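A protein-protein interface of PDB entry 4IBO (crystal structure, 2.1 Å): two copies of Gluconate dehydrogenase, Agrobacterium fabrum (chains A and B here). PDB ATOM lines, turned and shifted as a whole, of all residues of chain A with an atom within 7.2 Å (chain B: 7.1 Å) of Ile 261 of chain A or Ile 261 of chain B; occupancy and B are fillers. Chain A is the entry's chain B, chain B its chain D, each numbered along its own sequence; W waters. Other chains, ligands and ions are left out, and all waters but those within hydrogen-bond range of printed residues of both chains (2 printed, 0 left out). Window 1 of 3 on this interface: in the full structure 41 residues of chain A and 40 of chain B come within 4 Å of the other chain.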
ATOM      1  N   ASN A 201      12.712  -0.116 -29.232  1.00  0.00           N
ATOM      2  CA  ASN A 201      13.160   1.274 -29.266  1.00  0.00           C
ATOM      3  C   ASN A 201      14.549   1.345 -28.652  1.00  0.00           C
ATOM      4  O   ASN A 201      15.083   0.321 -28.210  1.00  0.00           O
ATOM      5  CB  ASN A 201      12.186   2.186 -28.522  1.00  0.00           C
ATOM      6  CG  ASN A 201      10.833   2.262 -29.199  1.00  0.00           C
ATOM      7  OD1 ASN A 201      10.688   2.908 -30.242  1.00  0.00           O
ATOM      8  ND2 ASN A 201       9.825   1.613 -28.603  1.00  0.00           N
ATOM      9  N   ALA A 202      15.138   2.543 -28.632  1.00  0.00           N
ATOM     10  CA  ALA A 202      16.490   2.707 -28.094  1.00  0.00           C
ATOM     11  C   ALA A 202      16.640   3.967 -27.257  1.00  0.00           C
ATOM     12  O   ALA A 202      15.882   4.932 -27.421  1.00  0.00           O
ATOM     13  CB  ALA A 202      17.519   2.709 -29.224  1.00  0.00           C
ATOM     14  N   ILE A 203      17.625   3.953 -26.364  1.00  0.00           N
ATOM     15  CA  ILE A 203      17.996   5.136 -25.592  1.00  0.00           C
ATOM     16  C   ILE A 203      19.432   5.484 -25.992  1.00  0.00           C
ATOM     17  O   ILE A 203      20.307   4.599 -26.063  1.00  0.00           O
ATOM     18  CB  ILE A 203      17.952   4.854 -24.079  1.00  0.00           C
ATOM     19  CG1 ILE A 203      16.562   4.369 -23.645  1.00  0.00           C
ATOM     20  CG2 ILE A 203      18.364   6.085 -23.273  1.00  0.00           C
ATOM     21  CD1 ILE A 203      16.509   3.947 -22.173  1.00  0.00           C
ATOM     22  N   GLY A 204      19.688   6.756 -26.270  1.00  0.00           N
ATOM     23  CA  GLY A 204      21.056   7.191 -26.520  1.00  0.00           C
ATOM     24  C   GLY A 204      21.517   8.095 -25.389  1.00  0.00           C
ATOM     25  O   GLY A 204      21.193   9.281 -25.377  1.00  0.00           O
ATOM     26  N   PRO A 205      22.241   7.533 -24.409  1.00  0.00           N
ATOM     27  CA  PRO A 205      22.728   8.350 -23.292  1.00  0.00           C
ATOM     28  C   PRO A 205      23.801   9.309 -23.771  1.00  0.00           C
ATOM     29  O   PRO A 205      24.623   8.952 -24.622  1.00  0.00           O
ATOM     30  CB  PRO A 205      23.360   7.322 -22.338  1.00  0.00           C
ATOM     31  CG  PRO A 205      22.786   5.984 -22.756  1.00  0.00           C
ATOM     32  CD  PRO A 205      22.579   6.109 -24.247  1.00  0.00           C
ATOM     33  N   LEU A 241      18.347   8.519 -16.734  1.00  0.00           N
ATOM     34  CA  LEU A 241      17.965   7.591 -17.805  1.00  0.00           C
ATOM     35  C   LEU A 241      16.696   6.824 -17.445  1.00  0.00           C
ATOM     36  O   LEU A 241      16.072   6.203 -18.306  1.00  0.00           O
ATOM     37  CB  LEU A 241      19.075   6.568 -18.062  1.00  0.00           C
ATOM     38  CG  LEU A 241      20.396   7.117 -18.583  1.00  0.00           C
ATOM     39  CD1 LEU A 241      21.364   5.984 -18.855  1.00  0.00           C
ATOM     40  CD2 LEU A 241      20.137   7.930 -19.844  1.00  0.00           C
ATOM     41  N   THR A 244      13.162   7.578 -19.156  1.00  0.00           N
ATOM     42  CA  THR A 244      13.123   7.118 -20.541  1.00  0.00           C
ATOM     43  C   THR A 244      13.017   5.587 -20.595  1.00  0.00           C
ATOM     44  O   THR A 244      12.226   5.034 -21.367  1.00  0.00           O
ATOM     45  CB  THR A 244      14.352   7.616 -21.325  1.00  0.00           C
ATOM     46  OG1 THR A 244      14.431   9.045 -21.222  1.00  0.00           O
ATOM     47  CG2 THR A 244      14.240   7.252 -22.787  1.00  0.00           C
ATOM     48  N   PHE A 247       9.414   4.653 -19.496  1.00  0.00           N
ATOM     49  CA  PHE A 247       8.552   5.029 -20.616  1.00  0.00           C
ATOM     50  C   PHE A 247       8.589   3.973 -21.720  1.00  0.00           C
ATOM     51  O   PHE A 247       7.549   3.471 -22.143  1.00  0.00           O
ATOM     52  CB  PHE A 247       8.996   6.396 -21.163  1.00  0.00           C
ATOM     53  CG  PHE A 247       8.363   6.773 -22.476  1.00  0.00           C
ATOM     54  CD1 PHE A 247       6.977   6.855 -22.602  1.00  0.00           C
ATOM     55  CD2 PHE A 247       9.153   7.089 -23.576  1.00  0.00           C
ATOM     56  CE1 PHE A 247       6.392   7.219 -23.814  1.00  0.00           C
ATOM     57  CE2 PHE A 247       8.569   7.460 -24.799  1.00  0.00           C
ATOM     58  CZ  PHE A 247       7.189   7.525 -24.910  1.00  0.00           C
ATOM     59  N   LEU A 248       9.791   3.601 -22.151  1.00  0.00           N
ATOM     60  CA  LEU A 248       9.941   2.654 -23.253  1.00  0.00           C
ATOM     61  C   LEU A 248       9.641   1.194 -22.865  1.00  0.00           C
ATOM     62  O   LEU A 248       9.587   0.316 -23.736  1.00  0.00           O
ATOM     63  CB  LEU A 248      11.342   2.776 -23.869  1.00  0.00           C
ATOM     64  CG  LEU A 248      11.654   4.071 -24.623  1.00  0.00           C
ATOM     65  CD1 LEU A 248      13.056   3.984 -25.202  1.00  0.00           C
ATOM     66  CD2 LEU A 248      10.618   4.368 -25.737  1.00  0.00           C
ATOM     67  N   VAL A 256       4.890   3.450 -29.845  1.00  0.00           N
ATOM     68  CA  VAL A 256       6.209   3.976 -30.152  1.00  0.00           C
ATOM     69  C   VAL A 256       7.057   2.785 -30.627  1.00  0.00           C
ATOM     70  O   VAL A 256       7.174   1.782 -29.919  1.00  0.00           O
ATOM     71  CB  VAL A 256       6.817   4.645 -28.902  1.00  0.00           C
ATOM     72  CG1 VAL A 256       8.159   5.248 -29.212  1.00  0.00           C
ATOM     73  CG2 VAL A 256       5.855   5.719 -28.350  1.00  0.00           C
ATOM     74  N   GLN A 259      12.160   4.008 -32.449  1.00  0.00           N
ATOM     75  CA  GLN A 259      12.674   5.325 -32.083  1.00  0.00           C
ATOM     76  C   GLN A 259      13.961   5.202 -31.295  1.00  0.00           C
ATOM     77  O   GLN A 259      14.116   4.273 -30.509  1.00  0.00           O
ATOM     78  CB  GLN A 259      11.650   6.032 -31.206  1.00  0.00           C
ATOM     79  CG  GLN A 259      10.378   6.375 -31.946  1.00  0.00           C
ATOM     80  CD  GLN A 259      10.651   7.409 -33.007  1.00  0.00           C
ATOM     81  OE1 GLN A 259      10.978   8.556 -32.689  1.00  0.00           O
ATOM     82  NE2 GLN A 259      10.563   7.007 -34.276  1.00  0.00           N
ATOM     83  N   ILE A 260      14.885   6.137 -31.483  1.00  0.00           N
ATOM     84  CA  ILE A 260      15.954   6.294 -30.497  1.00  0.00           C
ATOM     85  C   ILE A 260      15.807   7.642 -29.807  1.00  0.00           C
ATOM     86  O   ILE A 260      15.720   8.677 -30.461  1.00  0.00           O
ATOM     87  CB  ILE A 260      17.379   6.081 -31.095  1.00  0.00           C
ATOM     88  CG1 ILE A 260      18.442   6.287 -30.007  1.00  0.00           C
ATOM     89  CG2 ILE A 260      17.614   7.002 -32.283  1.00  0.00           C
ATOM     90  CD1 ILE A 260      19.848   5.916 -30.438  1.00  0.00           C
ATOM     91  N   ILE A 261      15.758   7.618 -28.480  1.00  0.00           N
ATOM     92  CA  ILE A 261      15.558   8.831 -27.700  1.00  0.00           C
ATOM     93  C   ILE A 261      16.875   9.183 -27.022  1.00  0.00           C
ATOM     94  O   ILE A 261      17.372   8.422 -26.181  1.00  0.00           O
ATOM     95  CB  ILE A 261      14.469   8.616 -26.615  1.00  0.00           C
ATOM     96  CG1 ILE A 261      13.115   8.293 -27.274  1.00  0.00           C
ATOM     97  CG2 ILE A 261      14.362   9.836 -25.703  1.00  0.00           C
ATOM     98  CD1 ILE A 261      11.994   8.023 -26.264  1.00  0.00           C
ATOM     99  N   TYR A 262      17.445  10.327 -27.392  1.00  0.00           N
ATOM    100  CA  TYR A 262      18.720  10.748 -26.829  1.00  0.00           C
ATOM    101  C   TYR A 262      18.481  11.479 -25.529  1.00  0.00           C
ATOM    102  O   TYR A 262      17.583  12.317 -25.441  1.00  0.00           O
ATOM    103  CB  TYR A 262      19.503  11.629 -27.818  1.00  0.00           C
ATOM    104  CG  TYR A 262      19.914  10.844 -29.038  1.00  0.00           C
ATOM    105  CD1 TYR A 262      20.996   9.969 -28.988  1.00  0.00           C
ATOM    106  CD2 TYR A 262      19.200  10.944 -30.220  1.00  0.00           C
ATOM    107  CE1 TYR A 262      21.360   9.215 -30.096  1.00  0.00           C
ATOM    108  CE2 TYR A 262      19.560  10.201 -31.337  1.00  0.00           C
ATOM    109  CZ  TYR A 262      20.639   9.337 -31.263  1.00  0.00           C
ATOM    110  OH  TYR A 262      21.002   8.602 -32.373  1.00  0.00           O
ATOM    111  N   VAL A 263      19.280  11.141 -24.520  1.00  0.00           N
ATOM    112  CA  VAL A 263      19.151  11.731 -23.199  1.00  0.00           C
ATOM    113  C   VAL A 263      20.487  12.413 -22.936  1.00  0.00           C
ATOM    114  O   VAL A 263      21.386  11.837 -22.319  1.00  0.00           O
ATOM    115  CB  VAL A 263      18.814  10.648 -22.150  1.00  0.00           C
ATOM    116  CG1 VAL A 263      18.548  11.272 -20.783  1.00  0.00           C
ATOM    117  CG2 VAL A 263      17.573   9.871 -22.601  1.00  0.00           C
ATOM    118  N   ASP A 264      20.613  13.640 -23.438  1.00  0.00           N
ATOM    119  CA  ASP A 264      21.928  14.232 -23.622  1.00  0.00           C
ATOM    120  C   ASP A 264      21.976  15.727 -23.369  1.00  0.00           C
ATOM    121  O   ASP A 264      22.912  16.388 -23.804  1.00  0.00           O
ATOM    122  CB  ASP A 264      22.459  13.937 -25.040  1.00  0.00           C
ATOM    123  CG  ASP A 264      21.698  14.690 -26.140  1.00  0.00           C
ATOM    124  OD1 ASP A 264      20.617  15.265 -25.873  1.00  0.00           O
ATOM    125  OD2 ASP A 264      22.184  14.693 -27.296  1.00  0.00           O
ATOM    126  N   ASN B 201      11.068  19.850 -26.323  1.00  0.00           N
ATOM    127  CA  ASN B 201      11.041  18.621 -27.104  1.00  0.00           C
ATOM    128  C   ASN B 201       9.789  18.613 -27.980  1.00  0.00           C
ATOM    129  O   ASN B 201       9.004  19.562 -27.957  1.00  0.00           O
ATOM    130  CB  ASN B 201      11.092  17.396 -26.183  1.00  0.00           C
ATOM    131  CG  ASN B 201      12.426  17.264 -25.472  1.00  0.00           C
ATOM    132  OD1 ASN B 201      13.442  16.995 -26.108  1.00  0.00           O
ATOM    133  ND2 ASN B 201      12.429  17.443 -24.150  1.00  0.00           N
ATOM    134  N   ALA B 202       9.616  17.562 -28.773  1.00  0.00           N
ATOM    135  CA  ALA B 202       8.495  17.506 -29.699  1.00  0.00           C
ATOM    136  C   ALA B 202       7.941  16.093 -29.820  1.00  0.00           C
ATOM    137  O   ALA B 202       8.650  15.110 -29.589  1.00  0.00           O
ATOM    138  CB  ALA B 202       8.897  18.048 -31.081  1.00  0.00           C
ATOM    139  N   ILE B 203       6.672  16.002 -30.192  1.00  0.00           N
ATOM    140  CA  ILE B 203       6.044  14.723 -30.477  1.00  0.00           C
ATOM    141  C   ILE B 203       5.611  14.712 -31.934  1.00  0.00           C
ATOM    142  O   ILE B 203       5.037  15.697 -32.418  1.00  0.00           O
ATOM    143  CB  ILE B 203       4.795  14.525 -29.621  1.00  0.00           C
ATOM    144  CG1 ILE B 203       5.151  14.581 -28.125  1.00  0.00           C
ATOM    145  CG2 ILE B 203       4.129  13.188 -29.946  1.00  0.00           C
ATOM    146  CD1 ILE B 203       3.934  14.570 -27.212  1.00  0.00           C
ATOM    147  N   GLY B 204       5.871  13.607 -32.633  1.00  0.00           N
ATOM    148  CA  GLY B 204       5.477  13.491 -34.026  1.00  0.00           C
ATOM    149  C   GLY B 204       4.457  12.380 -34.151  1.00  0.00           C
ATOM    150  O   GLY B 204       4.822  11.211 -34.313  1.00  0.00           O
ATOM    151  N   PRO B 205       3.168  12.728 -34.039  1.00  0.00           N
ATOM    152  CA  PRO B 205       2.134  11.696 -34.111  1.00  0.00           C
ATOM    153  C   PRO B 205       2.142  11.100 -35.500  1.00  0.00           C
ATOM    154  O   PRO B 205       2.396  11.828 -36.461  1.00  0.00           O
ATOM    155  CB  PRO B 205       0.840  12.482 -33.897  1.00  0.00           C
ATOM    156  CG  PRO B 205       1.275  13.740 -33.177  1.00  0.00           C
ATOM    157  CD  PRO B 205       2.600  14.064 -33.790  1.00  0.00           C
ATOM    158  N   LEU B 241      -0.882   9.015 -27.394  1.00  0.00           N
ATOM    159  CA  LEU B 241       0.063  10.134 -27.306  1.00  0.00           C
ATOM    160  C   LEU B 241       0.254  10.562 -25.850  1.00  0.00           C
ATOM    161  O   LEU B 241       1.194  11.302 -25.536  1.00  0.00           O
ATOM    162  CB  LEU B 241      -0.445  11.348 -28.100  1.00  0.00           C
ATOM    163  CG  LEU B 241      -0.577  11.195 -29.617  1.00  0.00           C
ATOM    164  CD1 LEU B 241      -1.085  12.484 -30.249  1.00  0.00           C
ATOM    165  CD2 LEU B 241       0.759  10.803 -30.241  1.00  0.00           C
ATOM    166  N   THR B 244       3.720   9.801 -24.046  1.00  0.00           N
ATOM    167  CA  THR B 244       4.804  10.637 -24.544  1.00  0.00           C
ATOM    168  C   THR B 244       4.657  12.078 -24.048  1.00  0.00           C
ATOM    169  O   THR B 244       5.641  12.727 -23.689  1.00  0.00           O
ATOM    170  CB  THR B 244       4.858  10.603 -26.086  1.00  0.00           C
ATOM    171  OG1 THR B 244       4.898   9.237 -26.521  1.00  0.00           O
ATOM    172  CG2 THR B 244       6.104  11.322 -26.617  1.00  0.00           C
ATOM    173  N   PHE B 247       5.484  12.121 -20.279  1.00  0.00           N
ATOM    174  CA  PHE B 247       6.923  11.913 -20.170  1.00  0.00           C
ATOM    175  C   PHE B 247       7.684  13.210 -20.467  1.00  0.00           C
ATOM    176  O   PHE B 247       8.550  13.622 -19.682  1.00  0.00           O
ATOM    177  CB  PHE B 247       7.346  10.789 -21.114  1.00  0.00           C
ATOM    178  CG  PHE B 247       8.825  10.711 -21.370  1.00  0.00           C
ATOM    179  CD1 PHE B 247       9.709  10.368 -20.355  1.00  0.00           C
ATOM    180  CD2 PHE B 247       9.328  10.933 -22.645  1.00  0.00           C
ATOM    181  CE1 PHE B 247      11.075  10.275 -20.606  1.00  0.00           C
ATOM    182  CE2 PHE B 247      10.692  10.840 -22.901  1.00  0.00           C
ATOM    183  CZ  PHE B 247      11.564  10.512 -21.880  1.00  0.00           C
ATOM    184  N   LEU B 248       7.329  13.880 -21.564  1.00  0.00           N
ATOM    185  CA  LEU B 248       8.032  15.108 -21.952  1.00  0.00           C
ATOM    186  C   LEU B 248       7.657  16.317 -21.100  1.00  0.00           C
ATOM    187  O   LEU B 248       8.250  17.387 -21.253  1.00  0.00           O
ATOM    188  CB  LEU B 248       7.797  15.441 -23.426  1.00  0.00           C
ATOM    189  CG  LEU B 248       8.435  14.497 -24.443  1.00  0.00           C
ATOM    190  CD1 LEU B 248       8.076  14.925 -25.870  1.00  0.00           C
ATOM    191  CD2 LEU B 248       9.949  14.450 -24.264  1.00  0.00           C
ATOM    192  N   VAL B 256      16.371  15.402 -21.215  1.00  0.00           N
ATOM    193  CA  VAL B 256      16.002  15.206 -22.611  1.00  0.00           C
ATOM    194  C   VAL B 256      15.718  16.581 -23.203  1.00  0.00           C
ATOM    195  O   VAL B 256      14.871  17.318 -22.690  1.00  0.00           O
ATOM    196  CB  VAL B 256      14.736  14.326 -22.738  1.00  0.00           C
ATOM    197  CG1 VAL B 256      14.337  14.148 -24.197  1.00  0.00           C
ATOM    198  CG2 VAL B 256      14.949  12.950 -22.067  1.00  0.00           C
ATOM    199  N   GLN B 259      14.646  16.871 -28.632  1.00  0.00           N
ATOM    200  CA  GLN B 259      14.236  15.610 -29.255  1.00  0.00           C
ATOM    201  C   GLN B 259      12.840  15.678 -29.867  1.00  0.00           C
ATOM    202  O   GLN B 259      11.947  16.316 -29.313  1.00  0.00           O
ATOM    203  CB  GLN B 259      14.246  14.497 -28.206  1.00  0.00           C
ATOM    204  CG  GLN B 259      15.636  14.151 -27.714  1.00  0.00           C
ATOM    205  CD  GLN B 259      16.478  13.587 -28.818  1.00  0.00           C
ATOM    206  OE1 GLN B 259      17.321  14.288 -29.390  1.00  0.00           O
ATOM    207  NE2 GLN B 259      16.237  12.320 -29.157  1.00  0.00           N
ATOM    208  N   ILE B 260      12.646  15.017 -31.004  1.00  0.00           N
ATOM    209  CA  ILE B 260      11.292  14.740 -31.479  1.00  0.00           C
ATOM    210  C   ILE B 260      11.042  13.238 -31.360  1.00  0.00           C
ATOM    211  O   ILE B 260      11.823  12.424 -31.862  1.00  0.00           O
ATOM    212  CB  ILE B 260      11.044  15.262 -32.920  1.00  0.00           C
ATOM    213  CG1 ILE B 260       9.607  14.958 -33.386  1.00  0.00           C
ATOM    214  CG2 ILE B 260      12.084  14.719 -33.893  1.00  0.00           C
ATOM    215  CD1 ILE B 260       9.124  15.862 -34.549  1.00  0.00           C
ATOM    216  N   ILE B 261       9.977  12.865 -30.668  1.00  0.00           N
ATOM    217  CA  ILE B 261       9.671  11.445 -30.502  1.00  0.00           C
ATOM    218  C   ILE B 261       8.476  11.106 -31.380  1.00  0.00           C
ATOM    219  O   ILE B 261       7.386  11.662 -31.197  1.00  0.00           O
ATOM    220  CB  ILE B 261       9.330  11.100 -29.034  1.00  0.00           C
ATOM    221  CG1 ILE B 261      10.502  11.458 -28.113  1.00  0.00           C
ATOM    222  CG2 ILE B 261       8.965   9.615 -28.893  1.00  0.00           C
ATOM    223  CD1 ILE B 261      10.185  11.305 -26.621  1.00  0.00           C
ATOM    224  N   TYR B 262       8.677  10.215 -32.345  1.00  0.00           N
ATOM    225  CA  TYR B 262       7.593   9.847 -33.251  1.00  0.00           C
ATOM    226  C   TYR B 262       6.731   8.755 -32.612  1.00  0.00           C
ATOM    227  O   TYR B 262       7.248   7.825 -32.000  1.00  0.00           O
ATOM    228  CB  TYR B 262       8.150   9.428 -34.622  1.00  0.00           C
ATOM    229  CG  TYR B 262       8.832  10.580 -35.339  1.00  0.00           C
ATOM    230  CD1 TYR B 262       8.086  11.583 -35.948  1.00  0.00           C
ATOM    231  CD2 TYR B 262      10.214  10.679 -35.384  1.00  0.00           C
ATOM    232  CE1 TYR B 262       8.703  12.656 -36.591  1.00  0.00           C
ATOM    233  CE2 TYR B 262      10.844  11.741 -36.025  1.00  0.00           C
ATOM    234  CZ  TYR B 262      10.080  12.727 -36.622  1.00  0.00           C
ATOM    235  OH  TYR B 262      10.697  13.782 -37.253  1.00  0.00           O
ATOM    236  N   VAL B 263       5.414   8.895 -32.718  1.00  0.00           N
ATOM    237  CA  VAL B 263       4.496   7.904 -32.163  1.00  0.00           C
ATOM    238  C   VAL B 263       3.681   7.422 -33.344  1.00  0.00           C
ATOM    239  O   VAL B 263       2.606   7.961 -33.646  1.00  0.00           O
ATOM    240  CB  VAL B 263       3.608   8.513 -31.069  1.00  0.00           C
ATOM    241  CG1 VAL B 263       2.780   7.436 -30.395  1.00  0.00           C
ATOM    242  CG2 VAL B 263       4.490   9.215 -30.035  1.00  0.00           C
ATOM    243  N   ASP B 264       4.223   6.422 -34.036  1.00  0.00           N
ATOM    244  CA  ASP B 264       3.777   6.133 -35.391  1.00  0.00           C
ATOM    245  C   ASP B 264       3.774   4.653 -35.731  1.00  0.00           C
ATOM    246  O   ASP B 264       3.749   4.299 -36.906  1.00  0.00           O
ATOM    247  CB  ASP B 264       4.659   6.875 -36.395  1.00  0.00           C
ATOM    248  CG  ASP B 264       6.084   6.323 -36.464  1.00  0.00           C
ATOM    249  OD1 ASP B 264       6.496   5.500 -35.600  1.00  0.00           O
ATOM    250  OD2 ASP B 264       6.811   6.734 -37.399  1.00  0.00           O
HETATM  251  O   HOH W   1       9.370   5.192 -36.432  1.00  0.00           O
HETATM  252  O   HOH W   2      19.592  16.485 -28.375  1.00  0.00           O
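N of Ala 202 of chain A sits at hydrogen-bond distance from O of Gln 259 of chain A (2.7 Å). The backbone carbonyl oxygen (O) of Ala 202 of chain A lies within hydrogen-bond range of the backbone NH (N) of Ile 261 of chain A, at 2.9 Å. The side-chain amide oxygen of Asn 201 of chain A lies within hydrogen-bond range of the backbone NH of Gln 259 of chain A (2.9 Å). The backbone NH (N) of Gly 204 of chain A sits at hydrogen-bond distance from the backbone carbonyl oxygen (O) of Ile 261 of chain A (2.9 Å). The side-chain amide oxygen of Asn 201 of chain B lies within hydrogen-bond range of the backbone NH of Gln 259 of chain B (2.8 Å). N of Ala 202 of chain B is in hydrogen-bond range of O of Gln 259 of chain B.
The side-chain amide oxygen (OE1) of Gln 259 of chain A is in hydrogen-bond range of the backbone NH (N) of Tyr 262 of chain B (2.9 Å). The side-chain amide nitrogen (NE2) of Gln 259 of chain B sits close to the backbone NH (N) of Tyr 262 of chain A (2.9 Å).
Phe 247 of chain A touches its own counterpart, Phe 247 of chain B. Gln 259 of chain A touches Ile 261 of chain B, and with the chains exchanged Ile 261 of chain A touches Gln 259 of chain B. Ile 260 of chain A touches Gln 259 of chain B, but with the chains exchanged Gln 259 of chain A does not touch Ile 260 of chain B (4.04 Å). Ile 261 of chain A touches its own counterpart, Ile 261 of chain B. Positions printed for both chains: 201, 202, 203, 204, 205, 241, 244, 247, 248, 256, 259, 260, 261, 262, 263 and 264. Of the 11 pairs that touch across the chains among the printed residues, 10 have their exchanged pair printed and touching as well.
Along chain A the printed residues that touch a printed residue of chain B span positions 244 to 262. Of the 16 printed residues of chain B, 6 touch a printed residue of chain A. Hydrophobic or aromatic side chains of chain B within 4 Å of the printed part of chain A: Phe 247, Val 256, Ile 261 and Tyr 262.
Water W2 lies within hydrogen-bond range of OD1 of Asp 264 of chain A and OE1 of Gln 259 of chain B. Water W1 bridges the side-chain carboxylate (OD1) of Asp 264 of chain B (3.0 Å) and the side-chain amide nitrogen (NE2) of Gln 259 of chain A (3.1 Å).
Of the printed residues of chain B, Phe 247 of chain A touches Thr 244 (3.3 Å) and Phe 247 (3.96 Å). Printed residues of chain B within 4 Å of Ile 260 of chain A: Gln 259. Ile 261 of chain A touches two residues of chain B. Ala 202 of chain B touches none of the printed residues of chain A. Of the printed residues of chain A, Val 256 of chain B touches Tyr 262 (3.9 Å). Of the printed residues of chain A, Gln 259 of chain B touches Ile 260, Ile 261 and Tyr 262. Printed residues of chain A within 4 Å of Ile 261 of chain B: Gln 259 and Ile 261. The nearest printed residue of chain B that does not touch Ile 261 of chain A is Val 256 of chain B (4.6 Å). The nearest printed residue of chain B that does not touch Gln 259 of chain A is Ile 260 of chain B (4.04 Å).
Among the printed residues, pairs that only touch across the chains: Thr 244 of chain A with Phe 247 of chain B, Phe 247 of chain A with Thr 244 of chain B, Phe 247 of chain A with Phe 247 of chain B, Val 256 of chain A with Tyr 262 of chain B, Gln 259 of chain A with Ile 261 of chain B, Ile 260 of chain A with Gln 259 of chain B, Ile 261 of chain A with Gln 259 of chain B, Ile 261 of chain A with Ile 261 of chain B and Tyr 262 of chain A with Val 256 of chain B.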
